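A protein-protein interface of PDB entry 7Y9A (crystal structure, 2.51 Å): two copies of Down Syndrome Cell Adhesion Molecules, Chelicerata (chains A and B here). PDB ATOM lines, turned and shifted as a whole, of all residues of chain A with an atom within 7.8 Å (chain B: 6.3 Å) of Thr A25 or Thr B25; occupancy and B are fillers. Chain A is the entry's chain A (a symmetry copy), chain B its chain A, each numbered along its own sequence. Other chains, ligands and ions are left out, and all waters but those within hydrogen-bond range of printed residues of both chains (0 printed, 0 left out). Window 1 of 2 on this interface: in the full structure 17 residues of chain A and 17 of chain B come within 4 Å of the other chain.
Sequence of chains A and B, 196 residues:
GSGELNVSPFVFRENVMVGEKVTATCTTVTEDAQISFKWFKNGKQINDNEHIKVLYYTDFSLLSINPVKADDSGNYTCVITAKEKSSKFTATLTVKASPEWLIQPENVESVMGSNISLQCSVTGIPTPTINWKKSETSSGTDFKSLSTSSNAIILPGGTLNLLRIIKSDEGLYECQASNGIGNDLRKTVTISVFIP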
ATOM      1  N   VAL A   7     -24.151  15.193   1.869  1.00  0.00           N
ATOM      2  CA  VAL A   7     -24.700  14.430   2.984  1.00  0.00           C
ATOM      3  C   VAL A   7     -24.882  12.985   2.538  1.00  0.00           C
ATOM      4  O   VAL A   7     -25.535  12.716   1.523  1.00  0.00           O
ATOM      5  CB  VAL A   7     -26.031  15.040   3.452  1.00  0.00           C
ATOM      6  CG1 VAL A   7     -26.560  14.284   4.664  1.00  0.00           C
ATOM      7  CG2 VAL A   7     -25.853  16.517   3.768  1.00  0.00           C
ATOM      8  N   SER A   8     -24.302  12.055   3.285  1.00  0.00           N
ATOM      9  CA  SER A   8     -24.445  10.640   2.951  1.00  0.00           C
ATOM     10  C   SER A   8     -25.904  10.221   3.079  1.00  0.00           C
ATOM     11  O   SER A   8     -26.540  10.509   4.104  1.00  0.00           O
ATOM     12  CB  SER A   8     -23.569   9.788   3.867  1.00  0.00           C
ATOM     13  OG  SER A   8     -23.666   8.418   3.526  1.00  0.00           O
ATOM     14  N   PRO A   9     -26.479   9.545   2.081  1.00  0.00           N
ATOM     15  CA  PRO A   9     -27.903   9.201   2.155  1.00  0.00           C
ATOM     16  C   PRO A   9     -28.210   8.300   3.342  1.00  0.00           C
ATOM     17  O   PRO A   9     -27.407   7.450   3.734  1.00  0.00           O
ATOM     18  CB  PRO A   9     -28.177   8.482   0.825  1.00  0.00           C
ATOM     19  CG  PRO A   9     -27.057   8.928  -0.108  1.00  0.00           C
ATOM     20  CD  PRO A   9     -25.863   9.130   0.803  1.00  0.00           C
ATOM     21  N   PHE A  10     -29.393   8.506   3.916  1.00  0.00           N
ATOM     22  CA  PHE A  10     -29.905   7.675   4.996  1.00  0.00           C
ATOM     23  C   PHE A  10     -31.345   7.292   4.695  1.00  0.00           C
ATOM     24  O   PHE A  10     -32.086   8.047   4.059  1.00  0.00           O
ATOM     25  CB  PHE A  10     -29.826   8.387   6.356  1.00  0.00           C
ATOM     26  CG  PHE A  10     -30.506   9.728   6.383  1.00  0.00           C
ATOM     27  CD1 PHE A  10     -31.862   9.827   6.647  1.00  0.00           C
ATOM     28  CD2 PHE A  10     -29.785  10.889   6.151  1.00  0.00           C
ATOM     29  CE1 PHE A  10     -32.490  11.060   6.671  1.00  0.00           C
ATOM     30  CE2 PHE A  10     -30.406  12.125   6.177  1.00  0.00           C
ATOM     31  CZ  PHE A  10     -31.761  12.209   6.438  1.00  0.00           C
ATOM     32  N   VAL A  11     -31.739   6.112   5.166  1.00  0.00           N
ATOM     33  CA  VAL A  11     -33.071   5.580   4.915  1.00  0.00           C
ATOM     34  C   VAL A  11     -33.639   5.020   6.212  1.00  0.00           C
ATOM     35  O   VAL A  11     -32.907   4.525   7.074  1.00  0.00           O
ATOM     36  CB  VAL A  11     -33.052   4.488   3.819  1.00  0.00           C
ATOM     37  CG1 VAL A  11     -32.438   3.206   4.359  1.00  0.00           C
ATOM     38  CG2 VAL A  11     -34.464   4.225   3.295  1.00  0.00           C
ATOM     39  N   PHE A  12     -34.960   5.106   6.346  1.00  0.00           N
ATOM     40  CA  PHE A  12     -35.679   4.415   7.405  1.00  0.00           C
ATOM     41  C   PHE A  12     -36.077   3.026   6.917  1.00  0.00           C
ATOM     42  O   PHE A  12     -36.338   2.818   5.731  1.00  0.00           O
ATOM     43  CB  PHE A  12     -36.928   5.190   7.825  1.00  0.00           C
ATOM     44  CG  PHE A  12     -36.652   6.587   8.296  1.00  0.00           C
ATOM     45  CD1 PHE A  12     -36.067   6.819   9.532  1.00  0.00           C
ATOM     46  CD2 PHE A  12     -36.984   7.673   7.505  1.00  0.00           C
ATOM     47  CE1 PHE A  12     -35.818   8.110   9.964  1.00  0.00           C
ATOM     48  CE2 PHE A  12     -36.735   8.962   7.932  1.00  0.00           C
ATOM     49  CZ  PHE A  12     -36.154   9.181   9.164  1.00  0.00           C
ATOM     50  N   LYS A  21     -38.889   1.728  17.732  1.00  0.00           N
ATOM     51  CA  LYS A  21     -37.852   2.748  17.793  1.00  0.00           C
ATOM     52  C   LYS A  21     -37.335   3.035  16.392  1.00  0.00           C
ATOM     53  O   LYS A  21     -37.247   2.129  15.554  1.00  0.00           O
ATOM     54  CB  LYS A  21     -36.706   2.289  18.699  1.00  0.00           C
ATOM     55  CG  LYS A  21     -35.503   3.207  18.740  1.00  0.00           C
ATOM     56  CD  LYS A  21     -34.347   2.536  19.491  1.00  0.00           C
ATOM     57  CE  LYS A  21     -33.456   3.556  20.176  1.00  0.00           C
ATOM     58  NZ  LYS A  21     -32.051   3.494  19.663  1.00  0.00           N
ATOM     59  N   THR A  23     -34.230   5.325  14.257  1.00  0.00           N
ATOM     60  CA  THR A  23     -32.982   6.046  14.305  1.00  0.00           C
ATOM     61  C   THR A  23     -32.738   6.619  12.923  1.00  0.00           C
ATOM     62  O   THR A  23     -33.227   6.074  11.927  1.00  0.00           O
ATOM     63  CB  THR A  23     -31.825   5.103  14.707  1.00  0.00           C
ATOM     64  OG1 THR A  23     -31.875   3.910  13.907  1.00  0.00           O
ATOM     65  CG2 THR A  23     -31.920   4.671  16.179  1.00  0.00           C
ATOM     66  N   ALA A  24     -31.848   7.618  12.864  1.00  0.00           N
ATOM     67  CA  ALA A  24     -31.339   8.115  11.588  1.00  0.00           C
ATOM     68  C   ALA A  24     -29.965   8.727  11.812  1.00  0.00           C
ATOM     69  O   ALA A  24     -29.768   9.481  12.769  1.00  0.00           O
ATOM     70  CB  ALA A  24     -32.272   9.153  10.926  1.00  0.00           C
ATOM     71  N   THR A  25     -29.017   8.397  10.936  1.00  0.00           N
ATOM     72  CA  THR A  25     -27.627   8.804  11.099  1.00  0.00           C
ATOM     73  C   THR A  25     -27.240   9.709   9.939  1.00  0.00           C
ATOM     74  O   THR A  25     -27.450   9.359   8.773  1.00  0.00           O
ATOM     75  CB  THR A  25     -26.679   7.597  11.181  1.00  0.00           C
ATOM     76  OG1 THR A  25     -27.156   6.674  12.171  1.00  0.00           O
ATOM     77  CG2 THR A  25     -25.285   8.058  11.549  1.00  0.00           C
ATOM     78  N   CYS A  26     -26.673  10.866  10.269  1.00  0.00           N
ATOM     79  CA  CYS A  26     -26.261  11.861   9.293  1.00  0.00           C
ATOM     80  C   CYS A  26     -24.750  12.017   9.356  1.00  0.00           C
ATOM     81  O   CYS A  26     -24.186  12.220  10.438  1.00  0.00           O
ATOM     82  CB  CYS A  26     -26.943  13.200   9.559  1.00  0.00           C
ATOM     83  SG  CYS A  26     -26.634  14.447   8.316  1.00  0.00           S
ATOM     84  N   THR A  27     -24.104  11.914   8.201  1.00  0.00           N
ATOM     85  CA  THR A  27     -22.663  12.075   8.096  1.00  0.00           C
ATOM     86  C   THR A  27     -22.350  12.533   6.678  1.00  0.00           C
ATOM     87  O   THR A  27     -23.228  12.585   5.813  1.00  0.00           O
ATOM     88  CB  THR A  27     -21.921  10.778   8.436  1.00  0.00           C
ATOM     89  OG1 THR A  27     -20.508  11.014   8.397  1.00  0.00           O
ATOM     90  CG2 THR A  27     -22.280   9.681   7.455  1.00  0.00           C
ATOM     91  N   THR A  28     -21.087  12.870   6.447  1.00  0.00           N
ATOM     92  CA  THR A  28     -20.640  13.291   5.130  1.00  0.00           C
ATOM     93  C   THR A  28     -20.149  12.091   4.326  1.00  0.00           C
ATOM     94  O   THR A  28     -19.811  11.039   4.875  1.00  0.00           O
ATOM     95  CB  THR A  28     -19.528  14.335   5.242  1.00  0.00           C
ATOM     96  OG1 THR A  28     -18.556  13.902   6.202  1.00  0.00           O
ATOM     97  CG2 THR A  28     -20.099  15.677   5.672  1.00  0.00           C
ATOM     98  N   PHE A  37     -24.298  19.961  12.621  1.00  0.00           N
ATOM     99  CA  PHE A  37     -25.514  19.285  12.196  1.00  0.00           C
ATOM    100  C   PHE A  37     -26.760  19.978  12.729  1.00  0.00           C
ATOM    101  O   PHE A  37     -26.750  20.582  13.806  1.00  0.00           O
ATOM    102  CB  PHE A  37     -25.532  17.816  12.667  1.00  0.00           C
ATOM    103  CG  PHE A  37     -24.336  17.020  12.233  1.00  0.00           C
ATOM    104  CD1 PHE A  37     -24.314  16.404  10.996  1.00  0.00           C
ATOM    105  CD2 PHE A  37     -23.234  16.884  13.065  1.00  0.00           C
ATOM    106  CE1 PHE A  37     -23.217  15.673  10.591  1.00  0.00           C
ATOM    107  CE2 PHE A  37     -22.133  16.153  12.664  1.00  0.00           C
ATOM    108  CZ  PHE A  37     -22.126  15.546  11.425  1.00  0.00           C
ATOM    109  N   TRP A  39     -31.209  18.998  12.449  1.00  0.00           N
ATOM    110  CA  TRP A  39     -32.272  18.146  11.936  1.00  0.00           C
ATOM    111  C   TRP A  39     -33.563  18.942  11.807  1.00  0.00           C
ATOM    112  O   TRP A  39     -33.793  19.903  12.546  1.00  0.00           O
ATOM    113  CB  TRP A  39     -32.504  16.947  12.857  1.00  0.00           C
ATOM    114  CG  TRP A  39     -31.411  15.928  12.824  1.00  0.00           C
ATOM    115  CD1 TRP A  39     -30.276  15.919  13.580  1.00  0.00           C
ATOM    116  CD2 TRP A  39     -31.351  14.762  11.993  1.00  0.00           C
ATOM    117  NE1 TRP A  39     -29.512  14.820  13.272  1.00  0.00           N
ATOM    118  CE2 TRP A  39     -30.148  14.094  12.300  1.00  0.00           C
ATOM    119  CE3 TRP A  39     -32.196  14.219  11.021  1.00  0.00           C
ATOM    120  CZ2 TRP A  39     -29.769  12.912  11.668  1.00  0.00           C
ATOM    121  CZ3 TRP A  39     -31.819  13.046  10.395  1.00  0.00           C
ATOM    122  CH2 TRP A  39     -30.615  12.404  10.720  1.00  0.00           C
ATOM    123  N   ASP A  59     -18.093  13.795  13.943  1.00  0.00           N
ATOM    124  CA  ASP A  59     -18.240  13.494  12.525  1.00  0.00           C
ATOM    125  C   ASP A  59     -19.602  12.910  12.169  1.00  0.00           C
ATOM    126  O   ASP A  59     -19.804  12.500  11.020  1.00  0.00           O
ATOM    127  CB  ASP A  59     -17.135  12.534  12.076  1.00  0.00           C
ATOM    128  CG  ASP A  59     -16.871  11.424  13.086  1.00  0.00           C
ATOM    129  OD1 ASP A  59     -16.196  11.697  14.103  1.00  0.00           O
ATOM    130  OD2 ASP A  59     -17.331  10.280  12.865  1.00  0.00           O
ATOM    131  N   PHE A  60     -20.540  12.862  13.111  1.00  0.00           N
ATOM    132  CA  PHE A  60     -21.869  12.364  12.784  1.00  0.00           C
ATOM    133  C   PHE A  60     -22.875  12.840  13.821  1.00  0.00           C
ATOM    134  O   PHE A  60     -22.514  13.261  14.923  1.00  0.00           O
ATOM    135  CB  PHE A  60     -21.884  10.832  12.684  1.00  0.00           C
ATOM    136  CG  PHE A  60     -21.899  10.131  14.018  1.00  0.00           C
ATOM    137  CD1 PHE A  60     -20.729   9.975  14.744  1.00  0.00           C
ATOM    138  CD2 PHE A  60     -23.080   9.631  14.546  1.00  0.00           C
ATOM    139  CE1 PHE A  60     -20.735   9.334  15.970  1.00  0.00           C
ATOM    140  CE2 PHE A  60     -23.092   8.990  15.774  1.00  0.00           C
ATOM    141  CZ  PHE A  60     -21.917   8.840  16.486  1.00  0.00           C
ATOM    142  N   SER A  61     -24.148  12.768  13.438  1.00  0.00           N
ATOM    143  CA  SER A  61     -25.264  13.096  14.313  1.00  0.00           C
ATOM    144  C   SER A  61     -26.309  11.995  14.212  1.00  0.00           C
ATOM    145  O   SER A  61     -26.435  11.331  13.179  1.00  0.00           O
ATOM    146  CB  SER A  61     -25.892  14.448  13.950  1.00  0.00           C
ATOM    147  OG  SER A  61     -26.889  14.806  14.889  1.00  0.00           O
ATOM    148  N   LEU A  62     -27.061  11.806  15.294  1.00  0.00           N
ATOM    149  CA  LEU A  62     -28.072  10.759  15.360  1.00  0.00           C
ATOM    150  C   LEU A  62     -29.409  11.351  15.778  1.00  0.00           C
ATOM    151  O   LEU A  62     -29.492  12.058  16.788  1.00  0.00           O
ATOM    152  CB  LEU A  62     -27.661   9.653  16.340  1.00  0.00           C
ATOM    153  CG  LEU A  62     -28.548   8.407  16.342  1.00  0.00           C
ATOM    154  CD1 LEU A  62     -28.245   7.546  15.115  1.00  0.00           C
ATOM    155  CD2 LEU A  62     -28.370   7.602  17.622  1.00  0.00           C
ATOM    156  N   LEU A  63     -30.444  11.071  14.991  1.00  0.00           N
ATOM    157  CA  LEU A  63     -31.824  11.368  15.350  1.00  0.00           C
ATOM    158  C   LEU A  63     -32.452  10.103  15.921  1.00  0.00           C
ATOM    159  O   LEU A  63     -32.292   9.017  15.352  1.00  0.00           O
ATOM    160  CB  LEU A  63     -32.610  11.856  14.134  1.00  0.00           C
ATOM    161  CG  LEU A  63     -34.119  12.013  14.306  1.00  0.00           C
ATOM    162  CD1 LEU A  63     -34.443  13.249  15.137  1.00  0.00           C
ATOM    163  CD2 LEU A  63     -34.801  12.094  12.940  1.00  0.00           C
ATOM    164  N   SER A  64     -33.160  10.243  17.039  1.00  0.00           N
ATOM    165  CA  SER A  64     -33.732   9.101  17.745  1.00  0.00           C
ATOM    166  C   SER A  64     -35.179   9.402  18.104  1.00  0.00           C
ATOM    167  O   SER A  64     -35.460  10.398  18.780  1.00  0.00           O
ATOM    168  CB  SER A  64     -32.923   8.771  19.003  1.00  0.00           C
ATOM    169  OG  SER A  64     -33.239   7.480  19.494  1.00  0.00           O
ATOM    170  N   CYS A  78     -31.607  16.288   7.355  1.00  0.00           N
ATOM    171  CA  CYS A  78     -30.377  16.682   8.022  1.00  0.00           C
ATOM    172  C   CYS A  78     -29.644  17.696   7.155  1.00  0.00           C
ATOM    173  O   CYS A  78     -29.548  17.526   5.937  1.00  0.00           O
ATOM    174  CB  CYS A  78     -29.469  15.483   8.285  1.00  0.00           C
ATOM    175  SG  CYS A  78     -27.845  15.966   8.895  1.00  0.00           S
ATOM    176  N   PHE A  89     -29.911  16.230   3.196  1.00  0.00           N
ATOM    177  CA  PHE A  89     -30.538  15.018   2.698  1.00  0.00           C
ATOM    178  C   PHE A  89     -31.851  14.819   3.435  1.00  0.00           C
ATOM    179  O   PHE A  89     -31.936  15.064   4.642  1.00  0.00           O
ATOM    180  CB  PHE A  89     -29.655  13.784   2.877  1.00  0.00           C
ATOM    181  CG  PHE A  89     -30.141  12.598   2.098  1.00  0.00           C
ATOM    182  CD1 PHE A  89     -29.836  12.460   0.754  1.00  0.00           C
ATOM    183  CD2 PHE A  89     -30.927  11.632   2.703  1.00  0.00           C
ATOM    184  CE1 PHE A  89     -30.294  11.373   0.034  1.00  0.00           C
ATOM    185  CE2 PHE A  89     -31.386  10.544   1.990  1.00  0.00           C
ATOM    186  CZ  PHE A  89     -31.074  10.417   0.654  1.00  0.00           C
ATOM    187  N   SER B   8     -32.469  -3.847  13.899  1.00  0.00           N
ATOM    188  CA  SER B   8     -33.043  -2.959  12.890  1.00  0.00           C
ATOM    189  C   SER B   8     -32.190  -2.986  11.628  1.00  0.00           C
ATOM    190  O   SER B   8     -30.961  -2.839  11.713  1.00  0.00           O
ATOM    191  CB  SER B   8     -33.141  -1.535  13.432  1.00  0.00           C
ATOM    192  OG  SER B   8     -33.735  -0.673  12.479  1.00  0.00           O
ATOM    193  N   PRO B   9     -32.780  -3.168  10.445  1.00  0.00           N
ATOM    194  CA  PRO B   9     -31.967  -3.273   9.229  1.00  0.00           C
ATOM    195  C   PRO B   9     -31.163  -2.006   8.971  1.00  0.00           C
ATOM    196  O   PRO B   9     -31.604  -0.891   9.256  1.00  0.00           O
ATOM    197  CB  PRO B   9     -32.998  -3.514   8.117  1.00  0.00           C
ATOM    198  CG  PRO B   9     -34.236  -4.047   8.828  1.00  0.00           C
ATOM    199  CD  PRO B   9     -34.222  -3.360  10.179  1.00  0.00           C
ATOM    200  N   PHE B  10     -29.963  -2.200   8.429  1.00  0.00           N
ATOM    201  CA  PHE B  10     -29.095  -1.107   8.016  1.00  0.00           C
ATOM    202  C   PHE B  10     -28.561  -1.391   6.620  1.00  0.00           C
ATOM    203  O   PHE B  10     -28.365  -2.547   6.236  1.00  0.00           O
ATOM    204  CB  PHE B  10     -27.926  -0.901   8.992  1.00  0.00           C
ATOM    205  CG  PHE B  10     -27.104  -2.137   9.230  1.00  0.00           C
ATOM    206  CD1 PHE B  10     -26.061  -2.467   8.380  1.00  0.00           C
ATOM    207  CD2 PHE B  10     -27.373  -2.965  10.309  1.00  0.00           C
ATOM    208  CE1 PHE B  10     -25.305  -3.605   8.597  1.00  0.00           C
ATOM    209  CE2 PHE B  10     -26.618  -4.103  10.533  1.00  0.00           C
ATOM    210  CZ  PHE B  10     -25.583  -4.422   9.674  1.00  0.00           C
ATOM    211  N   THR B  23     -20.298   4.533   7.125  1.00  0.00           N
ATOM    212  CA  THR B  23     -20.806   4.357   8.463  1.00  0.00           C
ATOM    213  C   THR B  23     -21.811   3.224   8.420  1.00  0.00           C
ATOM    214  O   THR B  23     -22.414   2.965   7.372  1.00  0.00           O
ATOM    215  CB  THR B  23     -21.480   5.655   8.963  1.00  0.00           C
ATOM    216  OG1 THR B  23     -22.392   6.141   7.963  1.00  0.00           O
ATOM    217  CG2 THR B  23     -20.457   6.770   9.230  1.00  0.00           C
ATOM    218  N   ALA B  24     -22.101   2.666   9.603  1.00  0.00           N
ATOM    219  CA  ALA B  24     -23.210   1.728   9.756  1.00  0.00           C
ATOM    220  C   ALA B  24     -23.694   1.770  11.196  1.00  0.00           C
ATOM    221  O   ALA B  24     -22.883   1.759  12.126  1.00  0.00           O
ATOM    222  CB  ALA B  24     -22.835   0.280   9.372  1.00  0.00           C
ATOM    223  N   THR B  25     -25.013   1.828  11.379  1.00  0.00           N
ATOM    224  CA  THR B  25     -25.612   2.003  12.696  1.00  0.00           C
ATOM    225  C   THR B  25     -26.442   0.771  13.026  1.00  0.00           C
ATOM    226  O   THR B  25     -27.283   0.348  12.225  1.00  0.00           O
ATOM    227  CB  THR B  25     -26.475   3.272  12.773  1.00  0.00           C
ATOM    228  OG1 THR B  25     -25.722   4.398  12.299  1.00  0.00           O
ATOM    229  CG2 THR B  25     -26.909   3.517  14.201  1.00  0.00           C
ATOM    230  N   CYS B  26     -26.202   0.208  14.206  1.00  0.00           N
ATOM    231  CA  CYS B  26     -26.885  -0.986  14.676  1.00  0.00           C
ATOM    232  C   CYS B  26     -27.704  -0.633  15.907  1.00  0.00           C
ATOM    233  O   CYS B  26     -27.182  -0.037  16.857  1.00  0.00           O
ATOM    234  CB  CYS B  26     -25.885  -2.091  15.004  1.00  0.00           C
ATOM    235  SG  CYS B  26     -26.631  -3.659  15.431  1.00  0.00           S
ATOM    236  N   THR B  27     -28.982  -0.994  15.881  1.00  0.00           N
ATOM    237  CA  THR B  27     -29.882  -0.758  16.997  1.00  0.00           C
ATOM    238  C   THR B  27     -30.989  -1.801  16.929  1.00  0.00           C
ATOM    239  O   THR B  27     -31.086  -2.570  15.969  1.00  0.00           O
ATOM    240  CB  THR B  27     -30.456   0.663  16.972  1.00  0.00           C
ATOM    241  OG1 THR B  27     -31.269   0.868  18.135  1.00  0.00           O
ATOM    242  CG2 THR B  27     -31.288   0.884  15.725  1.00  0.00           C
ATOM    243  N   TRP B  39     -19.475  -6.312  16.128  1.00  0.00           N
ATOM    244  CA  TRP B  39     -19.462  -6.232  14.675  1.00  0.00           C
ATOM    245  C   TRP B  39     -18.547  -7.305  14.102  1.00  0.00           C
ATOM    246  O   TRP B  39     -17.579  -7.723  14.742  1.00  0.00           O
ATOM    247  CB  TRP B  39     -18.988  -4.856  14.206  1.00  0.00           C
ATOM    248  CG  TRP B  39     -19.970  -3.754  14.448  1.00  0.00           C
ATOM    249  CD1 TRP B  39     -20.097  -3.004  15.580  1.00  0.00           C
ATOM    250  CD2 TRP B  39     -20.963  -3.274  13.533  1.00  0.00           C
ATOM    251  NE1 TRP B  39     -21.107  -2.085  15.427  1.00  0.00           N
ATOM    252  CE2 TRP B  39     -21.656  -2.231  14.180  1.00  0.00           C
ATOM    253  CE3 TRP B  39     -21.333  -3.626  12.231  1.00  0.00           C
ATOM    254  CZ2 TRP B  39     -22.699  -1.538  13.571  1.00  0.00           C
ATOM    255  CZ3 TRP B  39     -22.367  -2.936  11.627  1.00  0.00           C
ATOM    256  CH2 TRP B  39     -23.040  -1.904  12.297  1.00  0.00           C
ATOM    257  N   PHE B  60     -27.212   1.982  20.953  1.00  0.00           N
ATOM    258  CA  PHE B  60     -26.799   1.806  19.568  1.00  0.00           C
ATOM    259  C   PHE B  60     -25.283   1.705  19.484  1.00  0.00           C
ATOM    260  O   PHE B  60     -24.560   2.082  20.410  1.00  0.00           O
ATOM    261  CB  PHE B  60     -27.310   2.951  18.681  1.00  0.00           C
ATOM    262  CG  PHE B  60     -26.516   4.225  18.807  1.00  0.00           C
ATOM    263  CD1 PHE B  60     -26.729   5.086  19.871  1.00  0.00           C
ATOM    264  CD2 PHE B  60     -25.556   4.561  17.862  1.00  0.00           C
ATOM    265  CE1 PHE B  60     -26.003   6.256  19.994  1.00  0.00           C
ATOM    266  CE2 PHE B  60     -24.825   5.732  17.981  1.00  0.00           C
ATOM    267  CZ  PHE B  60     -25.050   6.581  19.048  1.00  0.00           C
ATOM    268  N   SER B  61     -24.819   1.181  18.352  1.00  0.00           N
ATOM    269  CA  SER B  61     -23.401   1.075  18.043  1.00  0.00           C
ATOM    270  C   SER B  61     -23.167   1.580  16.627  1.00  0.00           C
ATOM    271  O   SER B  61     -24.051   1.502  15.769  1.00  0.00           O
ATOM    272  CB  SER B  61     -22.898  -0.368  18.174  1.00  0.00           C
ATOM    273  OG  SER B  61     -21.494  -0.427  17.995  1.00  0.00           O
ATOM    274  N   LEU B  62     -21.965   2.101  16.386  1.00  0.00           N
ATOM    275  CA  LEU B  62     -21.611   2.664  15.090  1.00  0.00           C
ATOM    276  C   LEU B  62     -20.321   2.037  14.584  1.00  0.00           C
ATOM    277  O   LEU B  62     -19.316   2.009  15.301  1.00  0.00           O
ATOM    278  CB  LEU B  62     -21.455   4.187  15.172  1.00  0.00           C
ATOM    279  CG  LEU B  62     -21.281   4.908  13.835  1.00  0.00           C
ATOM    280  CD1 LEU B  62     -22.626   5.002  13.112  1.00  0.00           C
ATOM    281  CD2 LEU B  62     -20.674   6.291  14.025  1.00  0.00           C
ATOM    282  N   LEU B  63     -20.362   1.526  13.357  1.00  0.00           N
ATOM    283  CA  LEU B  63     -19.176   1.086  12.635  1.00  0.00           C
ATOM    284  C   LEU B  63     -18.743   2.207  11.700  1.00  0.00           C
ATOM    285  O   LEU B  63     -19.578   2.797  11.005  1.00  0.00           O
ATOM    286  CB  LEU B  63     -19.463  -0.191  11.845  1.00  0.00           C
ATOM    287  CG  LEU B  63     -18.378  -0.660  10.878  1.00  0.00           C
ATOM    288  CD1 LEU B  63     -17.205  -1.272  11.635  1.00  0.00           C
ATOM    289  CD2 LEU B  63     -18.956  -1.668   9.885  1.00  0.00           C
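OG1 of Thr B27 is in hydrogen-bond range of NZ of Lys A21, at 3.1 Å. The side-chain hydroxyl (OG1) of Thr B25 sits at hydrogen-bond distance from the side-chain hydroxyl (OG1) of Thr A25 (2.7 Å).
The backbone NH (N) of Ser B8 lies within hydrogen-bond range of the backbone carbonyl oxygen (O) of Thr B27 (2.8 Å). N of Ser A8 lies within hydrogen-bond range of O of Thr A27, at 2.8 Å. The side-chain hydroxyl (OG1) of Thr A27 lies within hydrogen-bond range of the backbone carbonyl oxygen (O) of Asp A59 (3.1 Å). The side-chain sulfur (SG) of Cys A26 is disulfide-bonded to the side-chain sulfur (SG) of Cys A78.
Thr B27 touches Thr A23 (CG2 to OG1, 3.6 Å). CG2 of Thr A27 touches OG1 of Thr B23, at 3.6 Å. CE1 of Phe A60 touches CD2 of Leu B62, 3.6 Å away. Leu A62 touches Phe B60 (CD2 to CE1, 3.6 Å).
Printed residues of chain B within 4 Å of Lys A21: Thr B27. Printed residues of chain B within 4 Å of Thr A25: Thr B25 (2.7 Å). Of the printed residues of chain B, Phe A60 touches Leu B62 (3.6 Å). Printed residues of chain B within 4 Å of Leu A62: Phe B60 (3.6 Å). Phe B10 touches none of the printed residues of chain A. Printed residues of chain A within 4 Å of Thr B23: Thr A27. No residue of chain A comes within 4 Å of Ala B24. Thr B25 touches just one residue of chain A: Thr A25 (2.7 Å). Printed residues of chain A within 4 Å of Leu B62: Phe A60. The nearest residue of chain A that does not touch Thr B25 is Leu A62 (4.3 Å).
Of the 13 printed residues of chain B, 5 touch a printed residue of chain A. Hydrophobic or aromatic side chains of chain B that line the printed part of chain A: Phe B60 and Leu B62. Among the printed residues, 6 pairs touch across the chains.
Thr A23 touches Thr B27, and with the chains exchanged Thr A27 touches Thr B23. Thr B25 touches its own counterpart, Thr A25. Phe A60 touches Leu B62, and with the chains exchanged Leu A62 touches Phe B60. 13 positions are printed for both chains.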
